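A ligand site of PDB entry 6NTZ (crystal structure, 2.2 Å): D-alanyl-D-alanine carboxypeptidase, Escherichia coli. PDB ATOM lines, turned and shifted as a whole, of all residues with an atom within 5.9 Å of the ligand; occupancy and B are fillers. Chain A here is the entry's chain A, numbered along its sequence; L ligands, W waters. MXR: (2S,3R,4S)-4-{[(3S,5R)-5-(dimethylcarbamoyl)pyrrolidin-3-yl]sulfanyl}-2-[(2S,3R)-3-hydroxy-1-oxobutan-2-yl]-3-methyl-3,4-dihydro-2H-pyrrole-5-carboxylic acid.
O8 of the ligand sits at hydrogen-bond distance from ND2 of Asn 141 (3.1 Å).
OG of Ser 139 sits at hydrogen-bond distance from N10 of the ligand (3.3 Å).
The side-chain hydroxyl (OG) of Ser 73 is bonded to a carbon (C1) of the ligand, at 0.9 Å.
The guanidinium group (NH1) of Arg 277 lies within salt-bridge range of an oxygen (O13) of the ligand, 3.8 Å away.
OG1 of Thr 243 is in hydrogen-bond range of O12 of the ligand (3.2 Å).
N of Ser 73 lies within hydrogen-bond range of O6 of the ligand (2.5 Å).
NZ of Lys 242 is in salt-bridge range of O12 of the ligand (3.9 Å).
N of His 245 lies within hydrogen-bond range of O6 of the ligand, 3.0 Å away.
The backbone carbonyl oxygen (O) of Ser 116 lies within hydrogen-bond range of the side-chain amide nitrogen (ND2) of Asn 141, at 3.2 Å.
The side-chain hydroxyl (OG) of Ser 73 lies close to the side-chain hydroxyl (OG) of Ser 139 (3.4 Å).
O of Ser 139 is in hydrogen-bond range of OG of Ser 116.
The side-chain hydroxyl (OG) of Ser 73 sits at hydrogen-bond distance from the side-chain amino group (NZ) of Lys 76 (3.4 Å).
N of Leu 182 is in hydrogen-bond range of ND1 of His 180 (3.2 Å).
The side-chain hydroxyl (OG) of Ser 115 sits at hydrogen-bond distance from the side-chain amide nitrogen (ND2) of Asn 141 (2.9 Å).
The side-chain hydroxyl (OG) of Ser 116 sits at hydrogen-bond distance from the backbone carbonyl oxygen (O) of Gln 138, at 3.3 Å.
NH2 of Arg 277 sits at hydrogen-bond distance from O of Gly 244 (2.7 Å).
Water W2 lies within hydrogen-bond range of N of Arg 227 and O12 of the ligand.
Ala 72 touches the ligand (CB to O6, 3.3 Å).
Lys 76 touches the ligand.
O of Gly 114 touches C26 of the ligand (3.1 Å).
Ser 115 touches the ligand.
OG of Ser 116 touches C4 of the ligand (3.5 Å).
Gly 181 touches the ligand.
Leu 182 touches the ligand (N to C9, 3.9 Å).
Gly 244 touches the ligand (CA to O6, 3.3 Å).
Hydrophobic or aromatic side chains within 4 Å of the ligand: Ala 72 and Leu 182.
15 residues have an atom within 4 Å of the ligand: Ala 72, Ser 73, Lys 76, Gly 114, Ser 115, Ser 116, Ser 139, Asn 141, Gly 181, Leu 182, Lys 242, Thr 243, Gly 244, His 245 and Arg 277.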
ATOM      1  N   PRO A  71     -10.219  -4.268 -18.259  1.00  0.00           N
ATOM      2  CA  PRO A  71     -11.136  -3.952 -19.363  1.00  0.00           C
ATOM      3  C   PRO A  71     -10.766  -2.734 -20.203  1.00  0.00           C
ATOM      4  O   PRO A  71     -11.347  -2.570 -21.289  1.00  0.00           O
ATOM      5  CB  PRO A  71     -12.445  -3.699 -18.627  1.00  0.00           C
ATOM      6  CG  PRO A  71     -12.031  -3.106 -17.308  1.00  0.00           C
ATOM      7  CD  PRO A  71     -10.703  -3.757 -16.965  1.00  0.00           C
ATOM      8  N   ALA A  72      -9.868  -1.892 -19.712  1.00  0.00           N
ATOM      9  CA  ALA A  72      -9.490  -0.647 -20.358  1.00  0.00           C
ATOM     10  C   ALA A  72     -10.783   0.114 -20.651  1.00  0.00           C
ATOM     11  O   ALA A  72     -11.673   0.198 -19.791  1.00  0.00           O
ATOM     12  CB  ALA A  72      -8.635  -0.969 -21.561  1.00  0.00           C
ATOM     13  N   SER A  73     -10.943   0.649 -21.853  1.00  0.00           N
ATOM     14  CA  SER A  73     -12.079   1.525 -22.115  1.00  0.00           C
ATOM     15  C   SER A  73     -13.380   0.765 -22.301  1.00  0.00           C
ATOM     16  O   SER A  73     -14.420   1.402 -22.455  1.00  0.00           O
ATOM     17  CB  SER A  73     -11.776   2.377 -23.342  1.00  0.00           C
ATOM     18  OG  SER A  73     -10.527   3.038 -23.193  1.00  0.00           O
ATOM     19  N   LEU A  74     -13.357  -0.577 -22.308  1.00  0.00           N
ATOM     20  CA  LEU A  74     -14.601  -1.327 -22.219  1.00  0.00           C
ATOM     21  C   LEU A  74     -15.370  -0.981 -20.959  1.00  0.00           C
ATOM     22  O   LEU A  74     -16.587  -1.142 -20.909  1.00  0.00           O
ATOM     23  CB  LEU A  74     -14.346  -2.834 -22.252  1.00  0.00           C
ATOM     24  CG  LEU A  74     -13.669  -3.443 -23.487  1.00  0.00           C
ATOM     25  CD1 LEU A  74     -13.613  -4.966 -23.361  1.00  0.00           C
ATOM     26  CD2 LEU A  74     -14.368  -3.046 -24.776  1.00  0.00           C
ATOM     27  N   LYS A  76     -16.163   1.866 -20.207  1.00  0.00           N
ATOM     28  CA  LYS A  76     -17.133   2.869 -20.628  1.00  0.00           C
ATOM     29  C   LYS A  76     -18.434   2.272 -21.139  1.00  0.00           C
ATOM     30  O   LYS A  76     -19.421   3.008 -21.272  1.00  0.00           O
ATOM     31  CB  LYS A  76     -16.531   3.773 -21.696  1.00  0.00           C
ATOM     32  CG  LYS A  76     -15.349   4.596 -21.203  1.00  0.00           C
ATOM     33  CD  LYS A  76     -14.967   5.664 -22.209  1.00  0.00           C
ATOM     34  CE  LYS A  76     -13.681   6.374 -21.807  1.00  0.00           C
ATOM     35  NZ  LYS A  76     -12.496   5.459 -21.836  1.00  0.00           N
ATOM     36  N   GLY A 114      -1.901  11.362 -22.513  1.00  0.00           N
ATOM     37  CA  GLY A 114      -1.768  10.193 -23.356  1.00  0.00           C
ATOM     38  C   GLY A 114      -3.026   9.376 -23.492  1.00  0.00           C
ATOM     39  O   GLY A 114      -2.994   8.316 -24.127  1.00  0.00           O
ATOM     40  N   SER A 115      -4.132   9.825 -22.926  1.00  0.00           N
ATOM     41  CA  SER A 115      -5.409   9.158 -23.058  1.00  0.00           C
ATOM     42  C   SER A 115      -6.302   9.943 -24.007  1.00  0.00           C
ATOM     43  O   SER A 115      -6.067  11.125 -24.281  1.00  0.00           O
ATOM     44  CB  SER A 115      -6.073   9.005 -21.691  1.00  0.00           C
ATOM     45  OG  SER A 115      -6.622  10.236 -21.241  1.00  0.00           O
ATOM     46  N   SER A 116      -7.323   9.277 -24.536  1.00  0.00           N
ATOM     47  CA  SER A 116      -8.274   9.963 -25.395  1.00  0.00           C
ATOM     48  C   SER A 116      -9.173  10.873 -24.552  1.00  0.00           C
ATOM     49  O   SER A 116      -9.521  10.541 -23.412  1.00  0.00           O
ATOM     50  CB  SER A 116      -9.115   8.959 -26.185  1.00  0.00           C
ATOM     51  OG  SER A 116      -9.820   8.087 -25.327  1.00  0.00           O
ATOM     52  N   LEU A 117      -9.516  12.023 -25.115  1.00  0.00           N
ATOM     53  CA  LEU A 117     -10.324  13.036 -24.452  1.00  0.00           C
ATOM     54  C   LEU A 117     -11.122  13.766 -25.517  1.00  0.00           C
ATOM     55  O   LEU A 117     -10.720  13.839 -26.680  1.00  0.00           O
ATOM     56  CB  LEU A 117      -9.453  14.038 -23.685  1.00  0.00           C
ATOM     57  CG  LEU A 117      -8.463  13.527 -22.644  1.00  0.00           C
ATOM     58  CD1 LEU A 117      -7.199  14.382 -22.632  1.00  0.00           C
ATOM     59  CD2 LEU A 117      -9.111  13.488 -21.268  1.00  0.00           C
ATOM     60  N   GLN A 138     -15.589   8.794 -28.966  1.00  0.00           N
ATOM     61  CA  GLN A 138     -14.208   9.234 -28.817  1.00  0.00           C
ATOM     62  C   GLN A 138     -13.510   8.626 -27.608  1.00  0.00           C
ATOM     63  O   GLN A 138     -12.309   8.856 -27.428  1.00  0.00           O
ATOM     64  CB  GLN A 138     -14.146  10.765 -28.730  1.00  0.00           C
ATOM     65  CG  GLN A 138     -15.075  11.482 -29.703  1.00  0.00           C
ATOM     66  CD  GLN A 138     -15.014  13.001 -29.553  1.00  0.00           C
ATOM     67  OE1 GLN A 138     -14.981  13.531 -28.449  1.00  0.00           O
ATOM     68  NE2 GLN A 138     -15.006  13.703 -30.691  1.00  0.00           N
ATOM     69  N   SER A 139     -14.231   7.853 -26.795  1.00  0.00           N
ATOM     70  CA  SER A 139     -13.699   7.280 -25.560  1.00  0.00           C
ATOM     71  C   SER A 139     -13.121   8.352 -24.636  1.00  0.00           C
ATOM     72  O   SER A 139     -12.104   8.157 -23.972  1.00  0.00           O
ATOM     73  CB  SER A 139     -12.665   6.193 -25.850  1.00  0.00           C
ATOM     74  OG  SER A 139     -12.477   5.352 -24.715  1.00  0.00           O
ATOM     75  N   ASN A 141     -12.196  10.415 -21.714  1.00  0.00           N
ATOM     76  CA  ASN A 141     -12.188  10.187 -20.270  1.00  0.00           C
ATOM     77  C   ASN A 141     -12.665  11.411 -19.506  1.00  0.00           C
ATOM     78  O   ASN A 141     -13.272  11.262 -18.432  1.00  0.00           O
ATOM     79  CB  ASN A 141     -10.789   9.795 -19.808  1.00  0.00           C
ATOM     80  CG  ASN A 141     -10.279   8.569 -20.514  1.00  0.00           C
ATOM     81  OD1 ASN A 141     -10.995   7.580 -20.666  1.00  0.00           O
ATOM     82  ND2 ASN A 141      -9.031   8.623 -20.953  1.00  0.00           N
ATOM     83  N   HIS A 180     -14.036   5.824 -16.368  1.00  0.00           N
ATOM     84  CA  HIS A 180     -13.516   5.848 -17.726  1.00  0.00           C
ATOM     85  C   HIS A 180     -12.775   4.581 -18.131  1.00  0.00           C
ATOM     86  O   HIS A 180     -12.676   4.306 -19.334  1.00  0.00           O
ATOM     87  CB  HIS A 180     -12.577   7.048 -17.916  1.00  0.00           C
ATOM     88  CG  HIS A 180     -11.872   7.481 -16.662  1.00  0.00           C
ATOM     89  ND1 HIS A 180     -11.066   6.632 -15.929  1.00  0.00           N
ATOM     90  CD2 HIS A 180     -11.855   8.665 -16.005  1.00  0.00           C
ATOM     91  CE1 HIS A 180     -10.597   7.273 -14.877  1.00  0.00           C
ATOM     92  NE2 HIS A 180     -11.061   8.512 -14.893  1.00  0.00           N
ATOM     93  N   GLY A 181     -12.272   3.802 -17.195  1.00  0.00           N
ATOM     94  CA  GLY A 181     -11.456   2.672 -17.570  1.00  0.00           C
ATOM     95  C   GLY A 181      -9.975   2.948 -17.690  1.00  0.00           C
ATOM     96  O   GLY A 181      -9.248   2.111 -18.222  1.00  0.00           O
ATOM     97  N   LEU A 182      -9.521   4.110 -17.228  1.00  0.00           N
ATOM     98  CA  LEU A 182      -8.102   4.271 -16.970  1.00  0.00           C
ATOM     99  C   LEU A 182      -7.687   3.263 -15.891  1.00  0.00           C
ATOM    100  O   LEU A 182      -8.498   2.831 -15.069  1.00  0.00           O
ATOM    101  CB  LEU A 182      -7.774   5.707 -16.539  1.00  0.00           C
ATOM    102  CG  LEU A 182      -7.881   6.738 -17.674  1.00  0.00           C
ATOM    103  CD1 LEU A 182      -8.212   8.142 -17.170  1.00  0.00           C
ATOM    104  CD2 LEU A 182      -6.610   6.763 -18.502  1.00  0.00           C
ATOM    105  N   ASP A 183      -6.419   2.891 -15.919  1.00  0.00           N
ATOM    106  CA  ASP A 183      -5.953   1.699 -15.210  1.00  0.00           C
ATOM    107  C   ASP A 183      -6.048   1.910 -13.705  1.00  0.00           C
ATOM    108  O   ASP A 183      -5.324   2.740 -13.134  1.00  0.00           O
ATOM    109  CB  ASP A 183      -4.530   1.374 -15.652  1.00  0.00           C
ATOM    110  CG  ASP A 183      -4.454   1.016 -17.128  1.00  0.00           C
ATOM    111  OD1 ASP A 183      -5.487   1.152 -17.821  1.00  0.00           O
ATOM    112  OD2 ASP A 183      -3.358   0.637 -17.591  1.00  0.00           O
ATOM    113  N   GLN A 224     -12.758  13.133 -34.399  1.00  0.00           N
ATOM    114  CA  GLN A 224     -12.173  11.869 -33.969  1.00  0.00           C
ATOM    115  C   GLN A 224     -13.025  10.734 -34.490  1.00  0.00           C
ATOM    116  O   GLN A 224     -14.240  10.851 -34.617  1.00  0.00           O
ATOM    117  CB  GLN A 224     -12.047  11.801 -32.435  1.00  0.00           C
ATOM    118  CG  GLN A 224     -11.175  12.886 -31.847  1.00  0.00           C
ATOM    119  CD  GLN A 224     -11.042  12.788 -30.338  1.00  0.00           C
ATOM    120  OE1 GLN A 224     -11.586  13.624 -29.598  1.00  0.00           O
ATOM    121  NE2 GLN A 224     -10.331  11.767 -29.852  1.00  0.00           N
ATOM    122  N   ARG A 227     -12.987   4.070 -33.215  1.00  0.00           N
ATOM    123  CA  ARG A 227     -11.887   3.180 -33.534  1.00  0.00           C
ATOM    124  C   ARG A 227     -12.329   1.709 -33.699  1.00  0.00           C
ATOM    125  O   ARG A 227     -11.473   0.812 -33.692  1.00  0.00           O
ATOM    126  CB  ARG A 227     -10.786   3.299 -32.479  1.00  0.00           C
ATOM    127  CG  ARG A 227      -9.923   4.554 -32.644  1.00  0.00           C
ATOM    128  CD  ARG A 227      -8.864   4.402 -33.776  1.00  0.00           C
ATOM    129  NE  ARG A 227      -9.341   4.922 -35.059  1.00  0.00           N
ATOM    130  CZ  ARG A 227      -9.436   4.220 -36.178  1.00  0.00           C
ATOM    131  NH1 ARG A 227      -9.879   4.790 -37.306  1.00  0.00           N
ATOM    132  NH2 ARG A 227      -9.101   2.938 -36.175  1.00  0.00           N
ATOM    133  N   LYS A 242     -17.762  -1.324 -28.335  1.00  0.00           N
ATOM    134  CA  LYS A 242     -16.714  -0.500 -27.737  1.00  0.00           C
ATOM    135  C   LYS A 242     -15.333  -1.103 -27.916  1.00  0.00           C
ATOM    136  O   LYS A 242     -15.153  -2.319 -27.763  1.00  0.00           O
ATOM    137  CB  LYS A 242     -16.958  -0.294 -26.248  1.00  0.00           C
ATOM    138  CG  LYS A 242     -16.155   0.853 -25.659  1.00  0.00           C
ATOM    139  CD  LYS A 242     -16.669   2.180 -26.162  1.00  0.00           C
ATOM    140  CE  LYS A 242     -15.783   3.346 -25.702  1.00  0.00           C
ATOM    141  NZ  LYS A 242     -14.733   3.692 -26.706  1.00  0.00           N
ATOM    142  N   THR A 243     -14.363  -0.252 -28.216  1.00  0.00           N
ATOM    143  CA  THR A 243     -12.959  -0.620 -28.244  1.00  0.00           C
ATOM    144  C   THR A 243     -12.257  -0.180 -26.967  1.00  0.00           C
ATOM    145  O   THR A 243     -12.721   0.695 -26.221  1.00  0.00           O
ATOM    146  CB  THR A 243     -12.225  -0.015 -29.456  1.00  0.00           C
ATOM    147  OG1 THR A 243     -12.520   1.388 -29.547  1.00  0.00           O
ATOM    148  CG2 THR A 243     -12.614  -0.717 -30.747  1.00  0.00           C
ATOM    149  N   GLY A 244     -11.110  -0.795 -26.715  1.00  0.00           N
ATOM    150  CA  GLY A 244     -10.350  -0.535 -25.523  1.00  0.00           C
ATOM    151  C   GLY A 244      -8.947  -1.055 -25.702  1.00  0.00           C
ATOM    152  O   GLY A 244      -8.740  -2.106 -26.301  1.00  0.00           O
ATOM    153  N   HIS A 245      -7.977  -0.301 -25.198  1.00  0.00           N
ATOM    154  CA  HIS A 245      -6.587  -0.722 -25.341  1.00  0.00           C
ATOM    155  C   HIS A 245      -5.752   0.006 -24.299  1.00  0.00           C
ATOM    156  O   HIS A 245      -5.757   1.232 -24.242  1.00  0.00           O
ATOM    157  CB  HIS A 245      -6.073  -0.445 -26.739  1.00  0.00           C
ATOM    158  CG  HIS A 245      -4.610  -0.168 -26.802  1.00  0.00           C
ATOM    159  ND1 HIS A 245      -3.666  -1.039 -26.309  1.00  0.00           N
ATOM    160  CD2 HIS A 245      -3.922   0.905 -27.270  1.00  0.00           C
ATOM    161  CE1 HIS A 245      -2.461  -0.532 -26.480  1.00  0.00           C
ATOM    162  NE2 HIS A 245      -2.593   0.649 -27.056  1.00  0.00           N
ATOM    163  N   THR A 246      -5.066  -0.764 -23.454  1.00  0.00           N
ATOM    164  CA  THR A 246      -3.940  -0.269 -22.674  1.00  0.00           C
ATOM    165  C   THR A 246      -2.794  -1.249 -22.841  1.00  0.00           C
ATOM    166  O   THR A 246      -3.002  -2.399 -23.254  1.00  0.00           O
ATOM    167  CB  THR A 246      -4.290  -0.070 -21.189  1.00  0.00           C
ATOM    168  OG1 THR A 246      -4.426  -1.342 -20.542  1.00  0.00           O
ATOM    169  CG2 THR A 246      -5.581   0.722 -21.040  1.00  0.00           C
ATOM    170  N   ARG A 277      -7.083  -7.563 -33.322  1.00  0.00           N
ATOM    171  CA  ARG A 277      -8.312  -7.772 -32.563  1.00  0.00           C
ATOM    172  C   ARG A 277      -9.545  -7.713 -33.454  1.00  0.00           C
ATOM    173  O   ARG A 277     -10.521  -8.437 -33.214  1.00  0.00           O
ATOM    174  CB  ARG A 277      -8.418  -6.750 -31.423  1.00  0.00           C
ATOM    175  CG  ARG A 277      -8.950  -5.386 -31.833  1.00  0.00           C
ATOM    176  CD  ARG A 277      -8.922  -4.446 -30.654  1.00  0.00           C
ATOM    177  NE  ARG A 277      -8.966  -3.040 -31.049  1.00  0.00           N
ATOM    178  CZ  ARG A 277      -8.708  -2.041 -30.216  1.00  0.00           C
ATOM    179  NH1 ARG A 277      -8.776  -0.784 -30.628  1.00  0.00           N
ATOM    180  NH2 ARG A 277      -8.383  -2.308 -28.961  1.00  0.00           N
HETATM  181  C1  MXR L   1      -9.593   2.906 -23.297  1.00  0.00           C
HETATM  182  C2  MXR L   1      -7.621   3.957 -26.814  1.00  0.00           C
HETATM  183  C3  MXR L   1      -8.649   4.073 -23.477  1.00  0.00           C
HETATM  184  C4  MXR L   1      -8.728   4.838 -24.811  1.00  0.00           C
HETATM  185  C5  MXR L   1      -9.083   3.746 -26.736  1.00  0.00           C
HETATM  186  O6  MXR L   1      -9.233   1.750 -23.378  1.00  0.00           O
HETATM  187  C7  MXR L   1      -8.962   5.109 -22.425  1.00  0.00           C
HETATM  188  O8  MXR L   1      -8.051   6.147 -22.633  1.00  0.00           O
HETATM  189  C9  MXR L   1      -8.759   4.639 -21.003  1.00  0.00           C
HETATM  190  N10 MXR L   1      -9.592   4.106 -25.680  1.00  0.00           N
HETATM  191  C11 MXR L   1      -9.884   3.194 -27.776  1.00  0.00           C
HETATM  192  O12 MXR L   1     -11.049   3.737 -27.993  1.00  0.00           O
HETATM  193  O13 MXR L   1      -9.498   2.249 -28.425  1.00  0.00           O
HETATM  194  S14 MXR L   1      -7.211   4.509 -28.429  1.00  0.00           S
HETATM  195  C15 MXR L   1      -6.526   6.097 -28.646  1.00  0.00           C
HETATM  196  C16 MXR L   1      -5.218   6.266 -27.917  1.00  0.00           C
HETATM  197  C17 MXR L   1      -4.210   6.843 -28.895  1.00  0.00           C
HETATM  198  C18 MXR L   1      -7.442   4.857 -25.627  1.00  0.00           C
HETATM  199  N19 MXR L   1      -4.947   7.150 -30.115  1.00  0.00           N
HETATM  200  C20 MXR L   1      -6.330   4.281 -24.794  1.00  0.00           C
HETATM  201  C21 MXR L   1      -6.139   6.289 -30.102  1.00  0.00           C
HETATM  202  C22 MXR L   1      -3.600   8.067 -28.307  1.00  0.00           C
HETATM  203  N23 MXR L   1      -4.386   9.004 -27.817  1.00  0.00           N
HETATM  204  O24 MXR L   1      -2.403   8.150 -28.236  1.00  0.00           O
HETATM  205  C25 MXR L   1      -5.685   9.334 -28.337  1.00  0.00           C
HETATM  206  C26 MXR L   1      -3.991   9.792 -26.676  1.00  0.00           C
HETATM  207  O   HOH W   1      -5.572   5.301 -22.021  1.00  0.00           O
HETATM  208  O   HOH W   2     -13.048   4.824 -30.222  1.00  0.00           O
